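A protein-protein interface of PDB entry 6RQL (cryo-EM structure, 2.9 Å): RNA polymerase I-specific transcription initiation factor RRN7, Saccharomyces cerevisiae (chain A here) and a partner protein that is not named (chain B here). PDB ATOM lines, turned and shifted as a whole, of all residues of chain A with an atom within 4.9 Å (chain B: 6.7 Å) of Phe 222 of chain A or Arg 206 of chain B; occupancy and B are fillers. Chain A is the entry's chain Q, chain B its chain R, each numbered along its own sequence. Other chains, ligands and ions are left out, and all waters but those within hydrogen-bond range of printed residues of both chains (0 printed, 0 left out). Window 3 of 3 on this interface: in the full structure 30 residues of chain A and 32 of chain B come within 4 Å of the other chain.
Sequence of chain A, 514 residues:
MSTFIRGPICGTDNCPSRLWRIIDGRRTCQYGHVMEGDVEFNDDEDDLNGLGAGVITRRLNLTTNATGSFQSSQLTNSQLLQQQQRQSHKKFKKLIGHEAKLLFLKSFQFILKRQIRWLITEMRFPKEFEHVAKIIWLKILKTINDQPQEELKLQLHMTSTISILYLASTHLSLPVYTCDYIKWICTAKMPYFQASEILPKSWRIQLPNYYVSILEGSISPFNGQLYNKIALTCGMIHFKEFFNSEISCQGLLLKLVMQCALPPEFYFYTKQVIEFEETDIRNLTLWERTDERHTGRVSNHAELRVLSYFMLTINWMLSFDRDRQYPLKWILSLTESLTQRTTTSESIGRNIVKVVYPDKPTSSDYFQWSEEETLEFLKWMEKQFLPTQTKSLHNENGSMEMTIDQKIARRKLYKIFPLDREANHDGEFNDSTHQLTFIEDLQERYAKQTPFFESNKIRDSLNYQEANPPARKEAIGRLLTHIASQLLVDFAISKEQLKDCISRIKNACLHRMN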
ATOM      1  N   SER A 218      11.209  -3.909  20.196  1.00  0.00           N
ATOM      2  CA  SER A 218      10.090  -2.982  20.112  1.00  0.00           C
ATOM      3  C   SER A 218       9.247  -2.989  21.382  1.00  0.00           C
ATOM      4  O   SER A 218       8.711  -1.951  21.773  1.00  0.00           O
ATOM      5  CB  SER A 218       9.249  -3.313  18.890  1.00  0.00           C
ATOM      6  OG  SER A 218      10.028  -3.145  17.719  1.00  0.00           O
ATOM      7  N   ILE A 219       9.094  -4.142  22.030  1.00  0.00           N
ATOM      8  CA  ILE A 219       8.308  -4.251  23.255  1.00  0.00           C
ATOM      9  C   ILE A 219       9.120  -4.976  24.316  1.00  0.00           C
ATOM     10  O   ILE A 219      10.115  -5.641  24.020  1.00  0.00           O
ATOM     11  CB  ILE A 219       6.976  -4.995  23.039  1.00  0.00           C
ATOM     12  CG1 ILE A 219       7.255  -6.398  22.497  1.00  0.00           C
ATOM     13  CG2 ILE A 219       6.031  -4.204  22.147  1.00  0.00           C
ATOM     14  CD1 ILE A 219       6.058  -7.310  22.495  1.00  0.00           C
ATOM     15  N   SER A 220       8.686  -4.849  25.554  1.00  0.00           N
ATOM     16  CA  SER A 220       9.249  -5.694  26.589  1.00  0.00           C
ATOM     17  C   SER A 220       8.381  -6.937  26.768  1.00  0.00           C
ATOM     18  O   SER A 220       7.170  -6.892  26.530  1.00  0.00           O
ATOM     19  CB  SER A 220       9.345  -4.941  27.908  1.00  0.00           C
ATOM     20  OG  SER A 220       8.060  -4.723  28.448  1.00  0.00           O
ATOM     21  N   PRO A 221       8.977  -8.063  27.162  1.00  0.00           N
ATOM     22  CA  PRO A 221       8.183  -9.274  27.411  1.00  0.00           C
ATOM     23  C   PRO A 221       7.296  -9.095  28.631  1.00  0.00           C
ATOM     24  O   PRO A 221       7.744  -8.639  29.683  1.00  0.00           O
ATOM     25  CB  PRO A 221       9.245 -10.351  27.646  1.00  0.00           C
ATOM     26  CG  PRO A 221      10.467  -9.822  26.993  1.00  0.00           C
ATOM     27  CD  PRO A 221      10.420  -8.349  27.196  1.00  0.00           C
ATOM     28  N   PHE A 222       6.029  -9.459  28.480  1.00  0.00           N
ATOM     29  CA  PHE A 222       5.022  -9.124  29.469  1.00  0.00           C
ATOM     30  C   PHE A 222       4.036 -10.271  29.599  1.00  0.00           C
ATOM     31  O   PHE A 222       3.790 -11.004  28.637  1.00  0.00           O
ATOM     32  CB  PHE A 222       4.295  -7.821  29.099  1.00  0.00           C
ATOM     33  CG  PHE A 222       3.441  -7.917  27.858  1.00  0.00           C
ATOM     34  CD1 PHE A 222       4.006  -7.816  26.594  1.00  0.00           C
ATOM     35  CD2 PHE A 222       2.070  -8.038  27.959  1.00  0.00           C
ATOM     36  CE1 PHE A 222       3.225  -7.892  25.463  1.00  0.00           C
ATOM     37  CE2 PHE A 222       1.286  -8.104  26.833  1.00  0.00           C
ATOM     38  CZ  PHE A 222       1.866  -8.028  25.583  1.00  0.00           C
ATOM     39  N   ASN A 223       3.479 -10.399  30.809  1.00  0.00           N
ATOM     40  CA  ASN A 223       2.491 -11.418  31.180  1.00  0.00           C
ATOM     41  C   ASN A 223       3.010 -12.828  30.925  1.00  0.00           C
ATOM     42  O   ASN A 223       2.309 -13.674  30.367  1.00  0.00           O
ATOM     43  CB  ASN A 223       1.155 -11.195  30.476  1.00  0.00           C
ATOM     44  CG  ASN A 223       0.523  -9.882  30.853  1.00  0.00           C
ATOM     45  OD1 ASN A 223       0.686  -9.402  31.971  1.00  0.00           O
ATOM     46  ND2 ASN A 223      -0.234  -9.306  29.933  1.00  0.00           N
ATOM     47  N   GLY A 224       4.250 -13.078  31.332  1.00  0.00           N
ATOM     48  CA  GLY A 224       4.834 -14.396  31.192  1.00  0.00           C
ATOM     49  C   GLY A 224       5.196 -14.772  29.777  1.00  0.00           C
ATOM     50  O   GLY A 224       5.262 -15.959  29.458  1.00  0.00           O
ATOM     51  N   GLN A 225       5.422 -13.786  28.910  1.00  0.00           N
ATOM     52  CA  GLN A 225       5.847 -14.084  27.549  1.00  0.00           C
ATOM     53  C   GLN A 225       7.276 -14.606  27.521  1.00  0.00           C
ATOM     54  O   GLN A 225       7.637 -15.386  26.633  1.00  0.00           O
ATOM     55  CB  GLN A 225       5.686 -12.831  26.690  1.00  0.00           C
ATOM     56  CG  GLN A 225       6.019 -12.979  25.227  1.00  0.00           C
ATOM     57  CD  GLN A 225       5.534 -11.802  24.415  1.00  0.00           C
ATOM     58  OE1 GLN A 225       4.909 -10.884  24.946  1.00  0.00           O
ATOM     59  NE2 GLN A 225       5.818 -11.819  23.120  1.00  0.00           N
ATOM     60  N   TYR A 357       5.970  -1.125  32.261  1.00  0.00           N
ATOM     61  CA  TYR A 357       4.794  -1.984  32.220  1.00  0.00           C
ATOM     62  C   TYR A 357       3.537  -1.186  32.525  1.00  0.00           C
ATOM     63  O   TYR A 357       3.380  -0.707  33.653  1.00  0.00           O
ATOM     64  CB  TYR A 357       4.952  -3.144  33.192  1.00  0.00           C
ATOM     65  CG  TYR A 357       6.049  -4.063  32.734  1.00  0.00           C
ATOM     66  CD1 TYR A 357       5.815  -4.994  31.737  1.00  0.00           C
ATOM     67  CD2 TYR A 357       7.332  -3.960  33.252  1.00  0.00           C
ATOM     68  CE1 TYR A 357       6.817  -5.822  31.286  1.00  0.00           C
ATOM     69  CE2 TYR A 357       8.346  -4.785  32.808  1.00  0.00           C
ATOM     70  CZ  TYR A 357       8.081  -5.714  31.825  1.00  0.00           C
ATOM     71  OH  TYR A 357       9.075  -6.544  31.371  1.00  0.00           O
ATOM     72  N   PRO A 358       2.621  -1.021  31.567  1.00  0.00           N
ATOM     73  CA  PRO A 358       1.559  -0.022  31.704  1.00  0.00           C
ATOM     74  C   PRO A 358       0.234  -0.486  32.284  1.00  0.00           C
ATOM     75  O   PRO A 358      -0.569   0.379  32.657  1.00  0.00           O
ATOM     76  CB  PRO A 358       1.346   0.412  30.255  1.00  0.00           C
ATOM     77  CG  PRO A 358       1.575  -0.833  29.494  1.00  0.00           C
ATOM     78  CD  PRO A 358       2.665  -1.578  30.205  1.00  0.00           C
ATOM     79  N   ALA A 492       7.649 -10.011  35.294  1.00  0.00           N
ATOM     80  CA  ALA A 492       6.963  -9.784  34.016  1.00  0.00           C
ATOM     81  C   ALA A 492       5.804 -10.754  33.793  1.00  0.00           C
ATOM     82  O   ALA A 492       5.706 -11.415  32.760  1.00  0.00           O
ATOM     83  CB  ALA A 492       7.949  -9.830  32.845  1.00  0.00           C
ATOM     84  N   THR B 202      -3.115   6.463  24.718  1.00  0.00           N
ATOM     85  CA  THR B 202      -1.683   6.357  24.945  1.00  0.00           C
ATOM     86  C   THR B 202      -1.343   5.391  26.062  1.00  0.00           C
ATOM     87  O   THR B 202      -0.168   5.271  26.420  1.00  0.00           O
ATOM     88  CB  THR B 202      -1.096   7.719  25.292  1.00  0.00           C
ATOM     89  OG1 THR B 202      -1.524   8.089  26.605  1.00  0.00           O
ATOM     90  CG2 THR B 202      -1.612   8.746  24.337  1.00  0.00           C
ATOM     91  N   SER B 203      -2.331   4.717  26.639  1.00  0.00           N
ATOM     92  CA  SER B 203      -2.103   3.975  27.866  1.00  0.00           C
ATOM     93  C   SER B 203      -1.904   2.485  27.651  1.00  0.00           C
ATOM     94  O   SER B 203      -1.748   1.758  28.633  1.00  0.00           O
ATOM     95  CB  SER B 203      -3.259   4.197  28.838  1.00  0.00           C
ATOM     96  OG  SER B 203      -3.030   3.493  30.044  1.00  0.00           O
ATOM     97  N   GLU B 204      -1.914   2.009  26.412  1.00  0.00           N
ATOM     98  CA  GLU B 204      -1.640   0.609  26.117  1.00  0.00           C
ATOM     99  C   GLU B 204      -0.698   0.485  24.932  1.00  0.00           C
ATOM    100  O   GLU B 204      -0.701  -0.509  24.202  1.00  0.00           O
ATOM    101  CB  GLU B 204      -2.939  -0.159  25.884  1.00  0.00           C
ATOM    102  CG  GLU B 204      -3.773   0.298  24.692  1.00  0.00           C
ATOM    103  CD  GLU B 204      -4.745   1.392  25.049  1.00  0.00           C
ATOM    104  OE1 GLU B 204      -4.584   1.996  26.127  1.00  0.00           O
ATOM    105  OE2 GLU B 204      -5.670   1.649  24.254  1.00  0.00           O
ATOM    106  N   VAL B 205       0.155   1.486  24.746  1.00  0.00           N
ATOM    107  CA  VAL B 205       1.033   1.499  23.585  1.00  0.00           C
ATOM    108  C   VAL B 205       2.219   0.548  23.766  1.00  0.00           C
ATOM    109  O   VAL B 205       2.572  -0.181  22.831  1.00  0.00           O
ATOM    110  CB  VAL B 205       1.450   2.952  23.280  1.00  0.00           C
ATOM    111  CG1 VAL B 205       2.001   3.644  24.513  1.00  0.00           C
ATOM    112  CG2 VAL B 205       2.453   2.998  22.146  1.00  0.00           C
ATOM    113  N   ARG B 206       2.800   0.562  24.964  1.00  0.00           N
ATOM    114  CA  ARG B 206       3.861  -0.399  25.369  1.00  0.00           C
ATOM    115  C   ARG B 206       4.942  -0.505  24.296  1.00  0.00           C
ATOM    116  O   ARG B 206       5.393  -1.602  24.049  1.00  0.00           O
ATOM    117  CB  ARG B 206       3.296  -1.742  25.837  1.00  0.00           C
ATOM    118  CG  ARG B 206       2.704  -2.606  24.741  1.00  0.00           C
ATOM    119  CD  ARG B 206       2.771  -4.052  25.185  1.00  0.00           C
ATOM    120  NE  ARG B 206       1.691  -4.499  26.047  1.00  0.00           N
ATOM    121  CZ  ARG B 206       1.714  -4.505  27.374  1.00  0.00           C
ATOM    122  NH1 ARG B 206       2.771  -4.063  28.029  1.00  0.00           N
ATOM    123  NH2 ARG B 206       0.668  -4.954  28.043  1.00  0.00           N
ATOM    124  N   ASN B 207       5.348   0.622  23.729  1.00  0.00           N
ATOM    125  CA  ASN B 207       6.371   0.667  22.697  1.00  0.00           C
ATOM    126  C   ASN B 207       7.777   0.784  23.271  1.00  0.00           C
ATOM    127  O   ASN B 207       8.739   0.791  22.496  1.00  0.00           O
ATOM    128  CB  ASN B 207       6.095   1.860  21.772  1.00  0.00           C
ATOM    129  CG  ASN B 207       6.670   1.696  20.371  1.00  0.00           C
ATOM    130  OD1 ASN B 207       6.322   2.455  19.467  1.00  0.00           O
ATOM    131  ND2 ASN B 207       7.536   0.708  20.176  1.00  0.00           N
ATOM    132  N   TYR B 208       7.896   1.008  24.584  1.00  0.00           N
ATOM    133  CA  TYR B 208       9.110   1.196  25.387  1.00  0.00           C
ATOM    134  C   TYR B 208       9.827   2.513  25.089  1.00  0.00           C
ATOM    135  O   TYR B 208      10.546   3.037  25.945  1.00  0.00           O
ATOM    136  CB  TYR B 208      10.091   0.014  25.234  1.00  0.00           C
ATOM    137  CG  TYR B 208      11.371   0.205  26.013  1.00  0.00           C
ATOM    138  CD1 TYR B 208      11.383   0.090  27.390  1.00  0.00           C
ATOM    139  CD2 TYR B 208      12.546   0.582  25.380  1.00  0.00           C
ATOM    140  CE1 TYR B 208      12.534   0.308  28.112  1.00  0.00           C
ATOM    141  CE2 TYR B 208      13.699   0.807  26.095  1.00  0.00           C
ATOM    142  CZ  TYR B 208      13.685   0.665  27.462  1.00  0.00           C
ATOM    143  OH  TYR B 208      14.826   0.877  28.191  1.00  0.00           O
ATOM    144  N   ARG B 209       9.548   3.150  23.962  1.00  0.00           N
ATOM    145  CA  ARG B 209      10.130   4.453  23.713  1.00  0.00           C
ATOM    146  C   ARG B 209       9.099   5.540  23.922  1.00  0.00           C
ATOM    147  O   ARG B 209       9.398   6.576  24.514  1.00  0.00           O
ATOM    148  CB  ARG B 209      10.711   4.530  22.306  1.00  0.00           C
ATOM    149  CG  ARG B 209      11.550   5.760  22.090  1.00  0.00           C
ATOM    150  CD  ARG B 209      12.023   5.799  20.678  1.00  0.00           C
ATOM    151  NE  ARG B 209      10.889   5.972  19.787  1.00  0.00           N
ATOM    152  CZ  ARG B 209      10.949   5.801  18.477  1.00  0.00           C
ATOM    153  NH1 ARG B 209       9.866   5.978  17.733  1.00  0.00           N
ATOM    154  NH2 ARG B 209      12.093   5.443  17.915  1.00  0.00           N
ATOM    155  N   THR B 210       7.866   5.290  23.479  1.00  0.00           N
ATOM    156  CA  THR B 210       6.748   6.116  23.903  1.00  0.00           C
ATOM    157  C   THR B 210       6.509   5.976  25.392  1.00  0.00           C
ATOM    158  O   THR B 210       6.033   6.914  26.034  1.00  0.00           O
ATOM    159  CB  THR B 210       5.483   5.716  23.159  1.00  0.00           C
ATOM    160  OG1 THR B 210       5.075   4.429  23.613  1.00  0.00           O
ATOM    161  CG2 THR B 210       5.756   5.626  21.677  1.00  0.00           C
ATOM    162  N   ARG B 211       6.857   4.824  25.954  1.00  0.00           N
ATOM    163  CA  ARG B 211       6.596   4.549  27.353  1.00  0.00           C
ATOM    164  C   ARG B 211       7.517   5.346  28.265  1.00  0.00           C
ATOM    165  O   ARG B 211       7.184   5.557  29.433  1.00  0.00           O
ATOM    166  CB  ARG B 211       6.729   3.044  27.566  1.00  0.00           C
ATOM    167  CG  ARG B 211       6.226   2.484  28.863  1.00  0.00           C
ATOM    168  CD  ARG B 211       4.722   2.544  28.946  1.00  0.00           C
ATOM    169  NE  ARG B 211       4.276   3.664  29.759  1.00  0.00           N
ATOM    170  CZ  ARG B 211       3.021   4.091  29.817  1.00  0.00           C
ATOM    171  NH1 ARG B 211       2.092   3.512  29.075  1.00  0.00           N
ATOM    172  NH2 ARG B 211       2.701   5.109  30.602  1.00  0.00           N
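The backbone carbonyl oxygen of Ser 218 of chain A sits close to the side-chain amide nitrogen of Asn 207 of chain B (3.3 Å).
Ile 219 of chain A touches Arg 206 of chain B. Arg 206 of chain B touches Phe 222 of chain A. Ser 203 of chain B touches Pro 358 of chain A (O to CB, 3.7 Å). CD of Pro 358 of chain A touches NH1 of Arg 206 of chain B, 3.3 Å away. Pro 358 of chain A touches Arg 211 of chain B (CB to NH1, 3.4 Å).
Printed residues of chain B within 4 Å of Ser 218 of chain A: Asn 207 (2.8 Å). Phe 222 of chain A touches one residue of chain B. Thr 202 of chain B touches none of the printed residues of chain A. Of the printed residues of chain A, Arg 206 of chain B touches Ile 219 (3.3 Å), Phe 222 (3.4 Å) and Pro 358 (3.3 Å). Printed residues of chain A within 4 Å of Asn 207 of chain B: Ser 218 (2.8 Å). Thr 210 of chain B touches none of the printed residues of chain A. The nearest residue of chain A that does not touch Arg 206 of chain B is Ser 218 of chain A (4.04 Å).
Of the 11 printed residues of chain A, 4 touch a printed residue of chain B. Hydrophobic or aromatic side chains of chain A that line the printed part of chain B: Ile 219, Phe 222 and Pro 358. Along chain A the printed residues that touch a printed residue of chain B span positions 218 to 358. Among the printed residues, no Asp or Glu carboxylate lies within 4 Å of a Lys or Arg side-chain nitrogen of the other chain.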
